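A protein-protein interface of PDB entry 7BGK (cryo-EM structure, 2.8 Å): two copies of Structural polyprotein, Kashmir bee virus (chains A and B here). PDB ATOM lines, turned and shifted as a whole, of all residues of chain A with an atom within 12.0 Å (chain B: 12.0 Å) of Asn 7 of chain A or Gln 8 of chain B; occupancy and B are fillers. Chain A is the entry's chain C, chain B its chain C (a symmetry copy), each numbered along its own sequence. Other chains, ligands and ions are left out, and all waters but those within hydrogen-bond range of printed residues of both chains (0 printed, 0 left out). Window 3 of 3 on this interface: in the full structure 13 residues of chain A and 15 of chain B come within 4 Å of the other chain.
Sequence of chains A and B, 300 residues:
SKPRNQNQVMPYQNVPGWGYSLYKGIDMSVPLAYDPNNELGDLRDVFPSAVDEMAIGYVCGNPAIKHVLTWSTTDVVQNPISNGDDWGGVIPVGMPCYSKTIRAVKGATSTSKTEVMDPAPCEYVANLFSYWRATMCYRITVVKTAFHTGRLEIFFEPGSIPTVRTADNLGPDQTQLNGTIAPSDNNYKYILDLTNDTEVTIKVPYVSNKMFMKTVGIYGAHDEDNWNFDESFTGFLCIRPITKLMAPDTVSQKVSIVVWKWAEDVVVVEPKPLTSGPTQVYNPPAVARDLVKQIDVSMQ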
ATOM      1  N   SER A   1      -2.847  26.563  22.876  1.00  0.00           N
ATOM      2  CA  SER A   1      -3.324  26.710  24.269  1.00  0.00           C
ATOM      3  C   SER A   1      -4.708  26.121  24.395  1.00  0.00           C
ATOM      4  O   SER A   1      -5.041  25.485  25.389  1.00  0.00           O
ATOM      5  CB  SER A   1      -3.361  28.175  24.672  1.00  0.00           C
ATOM      6  OG  SER A   1      -4.430  28.834  24.027  1.00  0.00           O
ATOM      7  N   LYS A   2      -5.516  26.343  23.362  1.00  0.00           N
ATOM      8  CA  LYS A   2      -6.924  25.972  23.350  1.00  0.00           C
ATOM      9  C   LYS A   2      -7.129  24.917  22.273  1.00  0.00           C
ATOM     10  O   LYS A   2      -7.577  25.226  21.160  1.00  0.00           O
ATOM     11  CB  LYS A   2      -7.808  27.193  23.120  1.00  0.00           C
ATOM     12  CG  LYS A   2      -9.212  27.021  23.597  1.00  0.00           C
ATOM     13  CD  LYS A   2     -10.089  28.133  23.124  1.00  0.00           C
ATOM     14  CE  LYS A   2      -9.989  29.311  24.039  1.00  0.00           C
ATOM     15  NZ  LYS A   2     -10.901  29.180  25.167  1.00  0.00           N
ATOM     16  N   PRO A   3      -6.812  23.665  22.563  1.00  0.00           N
ATOM     17  CA  PRO A   3      -6.978  22.621  21.555  1.00  0.00           C
ATOM     18  C   PRO A   3      -8.434  22.309  21.277  1.00  0.00           C
ATOM     19  O   PRO A   3      -9.336  22.834  21.934  1.00  0.00           O
ATOM     20  CB  PRO A   3      -6.253  21.427  22.180  1.00  0.00           C
ATOM     21  CG  PRO A   3      -6.369  21.651  23.607  1.00  0.00           C
ATOM     22  CD  PRO A   3      -6.209  23.123  23.788  1.00  0.00           C
ATOM     23  N   ARG A   4      -8.666  21.446  20.302  1.00  0.00           N
ATOM     24  CA  ARG A   4     -10.005  21.091  19.883  1.00  0.00           C
ATOM     25  C   ARG A   4     -10.489  19.853  20.625  1.00  0.00           C
ATOM     26  O   ARG A   4      -9.742  19.186  21.341  1.00  0.00           O
ATOM     27  CB  ARG A   4     -10.033  20.856  18.381  1.00  0.00           C
ATOM     28  CG  ARG A   4     -11.209  21.482  17.684  1.00  0.00           C
ATOM     29  CD  ARG A   4     -11.268  21.021  16.261  1.00  0.00           C
ATOM     30  NE  ARG A   4     -10.226  21.622  15.433  1.00  0.00           N
ATOM     31  CZ  ARG A   4      -9.189  20.966  14.926  1.00  0.00           C
ATOM     32  NH1 ARG A   4      -9.022  19.678  15.155  1.00  0.00           N
ATOM     33  NH2 ARG A   4      -8.305  21.604  14.186  1.00  0.00           N
ATOM     34  N   ASN A   5     -11.766  19.548  20.442  1.00  0.00           N
ATOM     35  CA  ASN A   5     -12.384  18.400  21.079  1.00  0.00           C
ATOM     36  C   ASN A   5     -12.153  17.146  20.254  1.00  0.00           C
ATOM     37  O   ASN A   5     -12.302  17.154  19.029  1.00  0.00           O
ATOM     38  CB  ASN A   5     -13.882  18.637  21.253  1.00  0.00           C
ATOM     39  CG  ASN A   5     -14.596  17.443  21.820  1.00  0.00           C
ATOM     40  OD1 ASN A   5     -14.334  17.019  22.942  1.00  0.00           O
ATOM     41  ND2 ASN A   5     -15.512  16.895  21.050  1.00  0.00           N
ATOM     42  N   GLN A   6     -11.783  16.065  20.938  1.00  0.00           N
ATOM     43  CA  GLN A   6     -11.677  14.750  20.325  1.00  0.00           C
ATOM     44  C   GLN A   6     -12.622  13.750  20.971  1.00  0.00           C
ATOM     45  O   GLN A   6     -12.527  12.551  20.695  1.00  0.00           O
ATOM     46  CB  GLN A   6     -10.240  14.238  20.415  1.00  0.00           C
ATOM     47  CG  GLN A   6      -9.197  15.187  19.885  1.00  0.00           C
ATOM     48  CD  GLN A   6      -9.260  15.366  18.394  1.00  0.00           C
ATOM     49  OE1 GLN A   6      -9.822  14.547  17.684  1.00  0.00           O
ATOM     50  NE2 GLN A   6      -8.670  16.442  17.907  1.00  0.00           N
ATOM     51  N   ASN A   7     -13.524  14.216  21.824  1.00  0.00           N
ATOM     52  CA  ASN A   7     -14.503  13.361  22.465  1.00  0.00           C
ATOM     53  C   ASN A   7     -15.695  13.128  21.550  1.00  0.00           C
ATOM     54  O   ASN A   7     -16.021  13.953  20.692  1.00  0.00           O
ATOM     55  CB  ASN A   7     -14.957  13.973  23.782  1.00  0.00           C
ATOM     56  CG  ASN A   7     -13.824  14.144  24.757  1.00  0.00           C
ATOM     57  OD1 ASN A   7     -12.902  14.930  24.532  1.00  0.00           O
ATOM     58  ND2 ASN A   7     -13.889  13.419  25.857  1.00  0.00           N
ATOM     59  N   GLN A   8     -16.344  11.992  21.747  1.00  0.00           N
ATOM     60  CA  GLN A   8     -17.486  11.609  20.941  1.00  0.00           C
ATOM     61  C   GLN A   8     -18.770  12.208  21.491  1.00  0.00           C
ATOM     62  O   GLN A   8     -18.841  12.672  22.630  1.00  0.00           O
ATOM     63  CB  GLN A   8     -17.608  10.088  20.871  1.00  0.00           C
ATOM     64  CG  GLN A   8     -18.025   9.419  22.158  1.00  0.00           C
ATOM     65  CD  GLN A   8     -18.444   7.992  21.969  1.00  0.00           C
ATOM     66  OE1 GLN A   8     -17.614   7.100  21.812  1.00  0.00           O
ATOM     67  NE2 GLN A   8     -19.742   7.760  21.989  1.00  0.00           N
ATOM     68  N   VAL A   9     -19.793  12.192  20.645  1.00  0.00           N
ATOM     69  CA  VAL A   9     -21.136  12.584  21.043  1.00  0.00           C
ATOM     70  C   VAL A   9     -21.719  11.480  21.912  1.00  0.00           C
ATOM     71  O   VAL A   9     -21.812  10.322  21.492  1.00  0.00           O
ATOM     72  CB  VAL A   9     -22.001  12.854  19.809  1.00  0.00           C
ATOM     73  CG1 VAL A   9     -23.384  13.210  20.198  1.00  0.00           C
ATOM     74  CG2 VAL A   9     -21.405  13.965  18.998  1.00  0.00           C
ATOM     75  N   MET A  10     -22.090  11.825  23.118  1.00  0.00           N
ATOM     76  CA  MET A  10     -22.523  10.847  24.106  1.00  0.00           C
ATOM     77  C   MET A  10     -24.024  10.597  24.011  1.00  0.00           C
ATOM     78  O   MET A  10     -24.797  11.555  23.914  1.00  0.00           O
ATOM     79  CB  MET A  10     -22.191  11.331  25.505  1.00  0.00           C
ATOM     80  CG  MET A  10     -20.754  11.764  25.702  1.00  0.00           C
ATOM     81  SD  MET A  10     -19.570  10.555  25.095  1.00  0.00           S
ATOM     82  CE  MET A  10     -19.805   9.251  26.287  1.00  0.00           C
ATOM     83  N   PRO A  11     -24.474   9.345  24.043  1.00  0.00           N
ATOM     84  CA  PRO A  11     -25.910   9.069  24.103  1.00  0.00           C
ATOM     85  C   PRO A  11     -26.409   9.176  25.536  1.00  0.00           C
ATOM     86  O   PRO A  11     -25.638   9.336  26.480  1.00  0.00           O
ATOM     87  CB  PRO A  11     -26.013   7.643  23.577  1.00  0.00           C
ATOM     88  CG  PRO A  11     -24.756   7.031  23.978  1.00  0.00           C
ATOM     89  CD  PRO A  11     -23.702   8.095  23.952  1.00  0.00           C
ATOM     90  N   ARG B   4     -12.153  24.934  41.256  1.00  0.00           N
ATOM     91  CA  ARG B   4     -12.887  25.233  40.044  1.00  0.00           C
ATOM     92  C   ARG B   4     -12.908  24.024  39.118  1.00  0.00           C
ATOM     93  O   ARG B   4     -12.233  23.019  39.340  1.00  0.00           O
ATOM     94  CB  ARG B   4     -12.264  26.429  39.343  1.00  0.00           C
ATOM     95  CG  ARG B   4     -13.264  27.433  38.839  1.00  0.00           C
ATOM     96  CD  ARG B   4     -12.581  28.454  37.983  1.00  0.00           C
ATOM     97  NE  ARG B   4     -11.769  29.385  38.763  1.00  0.00           N
ATOM     98  CZ  ARG B   4     -10.442  29.427  38.748  1.00  0.00           C
ATOM     99  NH1 ARG B   4      -9.743  28.591  38.006  1.00  0.00           N
ATOM    100  NH2 ARG B   4      -9.805  30.312  39.488  1.00  0.00           N
ATOM    101  N   ASN B   5     -13.700  24.137  38.061  1.00  0.00           N
ATOM    102  CA  ASN B   5     -13.835  23.074  37.082  1.00  0.00           C
ATOM    103  C   ASN B   5     -12.733  23.168  36.041  1.00  0.00           C
ATOM    104  O   ASN B   5     -12.426  24.250  35.536  1.00  0.00           O
ATOM    105  CB  ASN B   5     -15.198  23.155  36.402  1.00  0.00           C
ATOM    106  CG  ASN B   5     -15.363  22.138  35.307  1.00  0.00           C
ATOM    107  OD1 ASN B   5     -15.336  20.935  35.548  1.00  0.00           O
ATOM    108  ND2 ASN B   5     -15.541  22.616  34.094  1.00  0.00           N
ATOM    109  N   GLN B   6     -12.138  22.019  35.726  1.00  0.00           N
ATOM    110  CA  GLN B   6     -11.179  21.908  34.638  1.00  0.00           C
ATOM    111  C   GLN B   6     -11.649  20.935  33.569  1.00  0.00           C
ATOM    112  O   GLN B   6     -10.875  20.588  32.673  1.00  0.00           O
ATOM    113  CB  GLN B   6      -9.818  21.469  35.174  1.00  0.00           C
ATOM    114  CG  GLN B   6      -9.283  22.308  36.305  1.00  0.00           C
ATOM    115  CD  GLN B   6      -8.900  23.699  35.883  1.00  0.00           C
ATOM    116  OE1 GLN B   6      -8.684  23.965  34.712  1.00  0.00           O
ATOM    117  NE2 GLN B   6      -8.804  24.598  36.847  1.00  0.00           N
ATOM    118  N   ASN B   7     -12.895  20.489  33.648  1.00  0.00           N
ATOM    119  CA  ASN B   7     -13.465  19.593  32.661  1.00  0.00           C
ATOM    120  C   ASN B   7     -13.969  20.371  31.456  1.00  0.00           C
ATOM    121  O   ASN B   7     -14.341  21.544  31.554  1.00  0.00           O
ATOM    122  CB  ASN B   7     -14.593  18.778  33.276  1.00  0.00           C
ATOM    123  CG  ASN B   7     -14.125  17.921  34.421  1.00  0.00           C
ATOM    124  OD1 ASN B   7     -13.711  18.426  35.467  1.00  0.00           O
ATOM    125  ND2 ASN B   7     -14.197  16.616  34.239  1.00  0.00           N
ATOM    126  N   GLN B   8     -13.981  19.701  30.315  1.00  0.00           N
ATOM    127  CA  GLN B   8     -14.409  20.307  29.071  1.00  0.00           C
ATOM    128  C   GLN B   8     -15.918  20.219  28.909  1.00  0.00           C
ATOM    129  O   GLN B   8     -16.605  19.457  29.589  1.00  0.00           O
ATOM    130  CB  GLN B   8     -13.717  19.641  27.882  1.00  0.00           C
ATOM    131  CG  GLN B   8     -14.162  18.228  27.593  1.00  0.00           C
ATOM    132  CD  GLN B   8     -13.710  17.735  26.251  1.00  0.00           C
ATOM    133  OE1 GLN B   8     -12.551  17.375  26.062  1.00  0.00           O
ATOM    134  NE2 GLN B   8     -14.627  17.708  25.303  1.00  0.00           N
ATOM    135  N   VAL B   9     -16.422  21.029  27.985  1.00  0.00           N
ATOM    136  CA  VAL B   9     -17.820  20.977  27.588  1.00  0.00           C
ATOM    137  C   VAL B   9     -18.031  19.730  26.741  1.00  0.00           C
ATOM    138  O   VAL B   9     -17.376  19.544  25.710  1.00  0.00           O
ATOM    139  CB  VAL B   9     -18.207  22.251  26.832  1.00  0.00           C
ATOM    140  CG1 VAL B   9     -19.615  22.193  26.380  1.00  0.00           C
ATOM    141  CG2 VAL B   9     -18.010  23.449  27.711  1.00  0.00           C
ATOM    142  N   MET B  10     -18.920  18.876  27.176  1.00  0.00           N
ATOM    143  CA  MET B  10     -19.117  17.576  26.552  1.00  0.00           C
ATOM    144  C   MET B  10     -20.145  17.656  25.428  1.00  0.00           C
ATOM    145  O   MET B  10     -21.203  18.265  25.612  1.00  0.00           O
ATOM    146  CB  MET B  10     -19.588  16.566  27.581  1.00  0.00           C
ATOM    147  CG  MET B  10     -18.739  16.491  28.832  1.00  0.00           C
ATOM    148  SD  MET B  10     -16.982  16.341  28.476  1.00  0.00           S
ATOM    149  CE  MET B  10     -16.931  14.689  27.809  1.00  0.00           C
ATOM    150  N   PRO B  11     -19.883  17.057  24.269  1.00  0.00           N
ATOM    151  CA  PRO B  11     -20.901  16.984  23.221  1.00  0.00           C
ATOM    152  C   PRO B  11     -21.851  15.827  23.485  1.00  0.00           C
ATOM    153  O   PRO B  11     -21.653  15.020  24.392  1.00  0.00           O
ATOM    154  CB  PRO B  11     -20.081  16.760  21.955  1.00  0.00           C
ATOM    155  CG  PRO B  11     -18.922  16.016  22.418  1.00  0.00           C
ATOM    156  CD  PRO B  11     -18.614  16.470  23.811  1.00  0.00           C
ATOM    157  N   TYR B  12     -22.901  15.751  22.674  1.00  0.00           N
ATOM    158  CA  TYR B  12     -24.064  15.013  23.139  1.00  0.00           C
ATOM    159  C   TYR B  12     -25.189  14.934  22.113  1.00  0.00           C
ATOM    160  O   TYR B  12     -25.247  15.692  21.143  1.00  0.00           O
ATOM    161  CB  TYR B  12     -24.511  15.701  24.397  1.00  0.00           C
ATOM    162  CG  TYR B  12     -25.848  15.345  24.904  1.00  0.00           C
ATOM    163  CD1 TYR B  12     -26.001  14.508  25.974  1.00  0.00           C
ATOM    164  CD2 TYR B  12     -26.971  15.899  24.330  1.00  0.00           C
ATOM    165  CE1 TYR B  12     -27.234  14.233  26.449  1.00  0.00           C
ATOM    166  CE2 TYR B  12     -28.205  15.627  24.796  1.00  0.00           C
ATOM    167  CZ  TYR B  12     -28.338  14.806  25.858  1.00  0.00           C
ATOM    168  OH  TYR B  12     -29.607  14.572  26.277  1.00  0.00           O
ATOM    169  N   GLN B  13     -26.108  14.007  22.388  1.00  0.00           N
ATOM    170  CA  GLN B  13     -27.319  13.758  21.624  1.00  0.00           C
ATOM    171  C   GLN B  13     -28.347  13.208  22.601  1.00  0.00           C
ATOM    172  O   GLN B  13     -28.038  12.284  23.357  1.00  0.00           O
ATOM    173  CB  GLN B  13     -27.054  12.762  20.494  1.00  0.00           C
ATOM    174  CG  GLN B  13     -28.168  12.597  19.513  1.00  0.00           C
ATOM    175  CD  GLN B  13     -27.824  11.624  18.418  1.00  0.00           C
ATOM    176  OE1 GLN B  13     -27.463  10.479  18.680  1.00  0.00           O
ATOM    177  NE2 GLN B  13     -27.934  12.069  17.181  1.00  0.00           N
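Of chain B, only Gln 8, Met 10 and Pro 11 come within 4 Å of Asn 7 of chain A. Gln 8 of chain B touches two residues of chain A. Asn 5 of chain A touches just these residues of chain B: Gln 8 (2.5 Å) and Pro 11 (3.8 Å). No residue of chain B comes within 4 Å of Gln 6 of chain A. Gln 8 of chain A touches just one residue of chain B: Pro 11 (3.4 Å). No residue of chain A comes within 4 Å of Asn 7 of chain B. Pro 11 of chain B touches just these residues of chain A: Asn 5 (3.8 Å), Asn 7 (3.96 Å), Gln 8 (3.4 Å) and Met 10 (3.5 Å). Printed residues of chain A within 4 Å of Tyr 12 of chain B: Val 9 (3.1 Å) and Met 10 (3.6 Å). Printed residues of chain B within 4 Å of Pro 11 of chain A: Gln 13. Of the printed residues of chain A, Gln 13 of chain B touches Val 9, Met 10 and Pro 11. Of the printed residues of chain B, Met 10 of chain A touches Pro 11 (3.5 Å), Tyr 12 (3.6 Å) and Gln 13 (3.2 Å). Asn 5 of chain B touches none of the printed residues of chain A. Lys 2 of chain A touches none of the printed residues of chain B. The nearest printed residue of chain B that does not touch Pro 11 of chain A is Tyr 12 of chain B (5.2 Å).
Asn 5 of chain A touches Gln 8 of chain B, but with the chains exchanged Gln 8 of chain A does not touch Asn 5 of chain B (15.5 Å). Asn 7 of chain A touches Met 10 of chain B, but with the chains exchanged Met 10 of chain A does not touch Asn 7 of chain B (11.8 Å). Asn 7 of chain A touches Pro 11 of chain B, but with the chains exchanged Pro 11 of chain A does not touch Asn 7 of chain B (15.6 Å). Gln 8 of chain A touches Pro 11 of chain B, but with the chains exchanged Pro 11 of chain A does not touch Gln 8 of chain B (13.0 Å). Positions printed for both chains: 4, 5, 6, 7, 8, 9, 10 and 11.
Printed residues of chain A that touch a printed residue of chain B: Asn 5, Asn 7, Gln 8, Val 9, Met 10 and Pro 11. Of the 10 printed residues of chain B, 5 touch a printed residue of chain A. Hydrophobic or aromatic side chains of chain B that line the printed part of chain A: Met 10, Pro 11 and Tyr 12.
OD1 of Asn 5 of chain A lies within hydrogen-bond range of NE2 of Gln 8 of chain B, 2.5 Å away. The backbone carbonyl oxygen (O) of Pro 11 of chain B lies within hydrogen-bond range of the backbone NH (N) of Met 10 of chain A (3.5 Å). The backbone NH (N) of Gln 13 of chain B lies within hydrogen-bond range of the backbone carbonyl oxygen (O) of Met 10 of chain A (3.2 Å). The side-chain amide oxygen of Asn 7 of chain A lies close to the side-chain amide oxygen of Gln 8 of chain B (2.9 Å).
CG of Pro 11 of chain B touches ND2 of Asn 5 of chain A (3.8 Å). Met 10 of chain B touches Asn 7 of chain A (CE to ND2, 3.8 Å). O of Asn 7 of chain A touches CG of Pro 11 of chain B (3.96 Å). CG of Pro 11 of chain B touches O of Gln 8 of chain A, at 3.4 Å. Val 9 of chain A touches Tyr 12 of chain B (CG1 to C, 3.1 Å). Val 9 of chain A touches Gln 13 of chain B. Tyr 12 of chain B touches Met 10 of chain A (CA to O, 3.6 Å). Pro 11 of chain A touches Gln 13 of chain B.
The side-chain amide oxygen of Asn 5 of chain A lies close to the side-chain amide oxygen of Asn 7 of chain A (3.0 Å).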
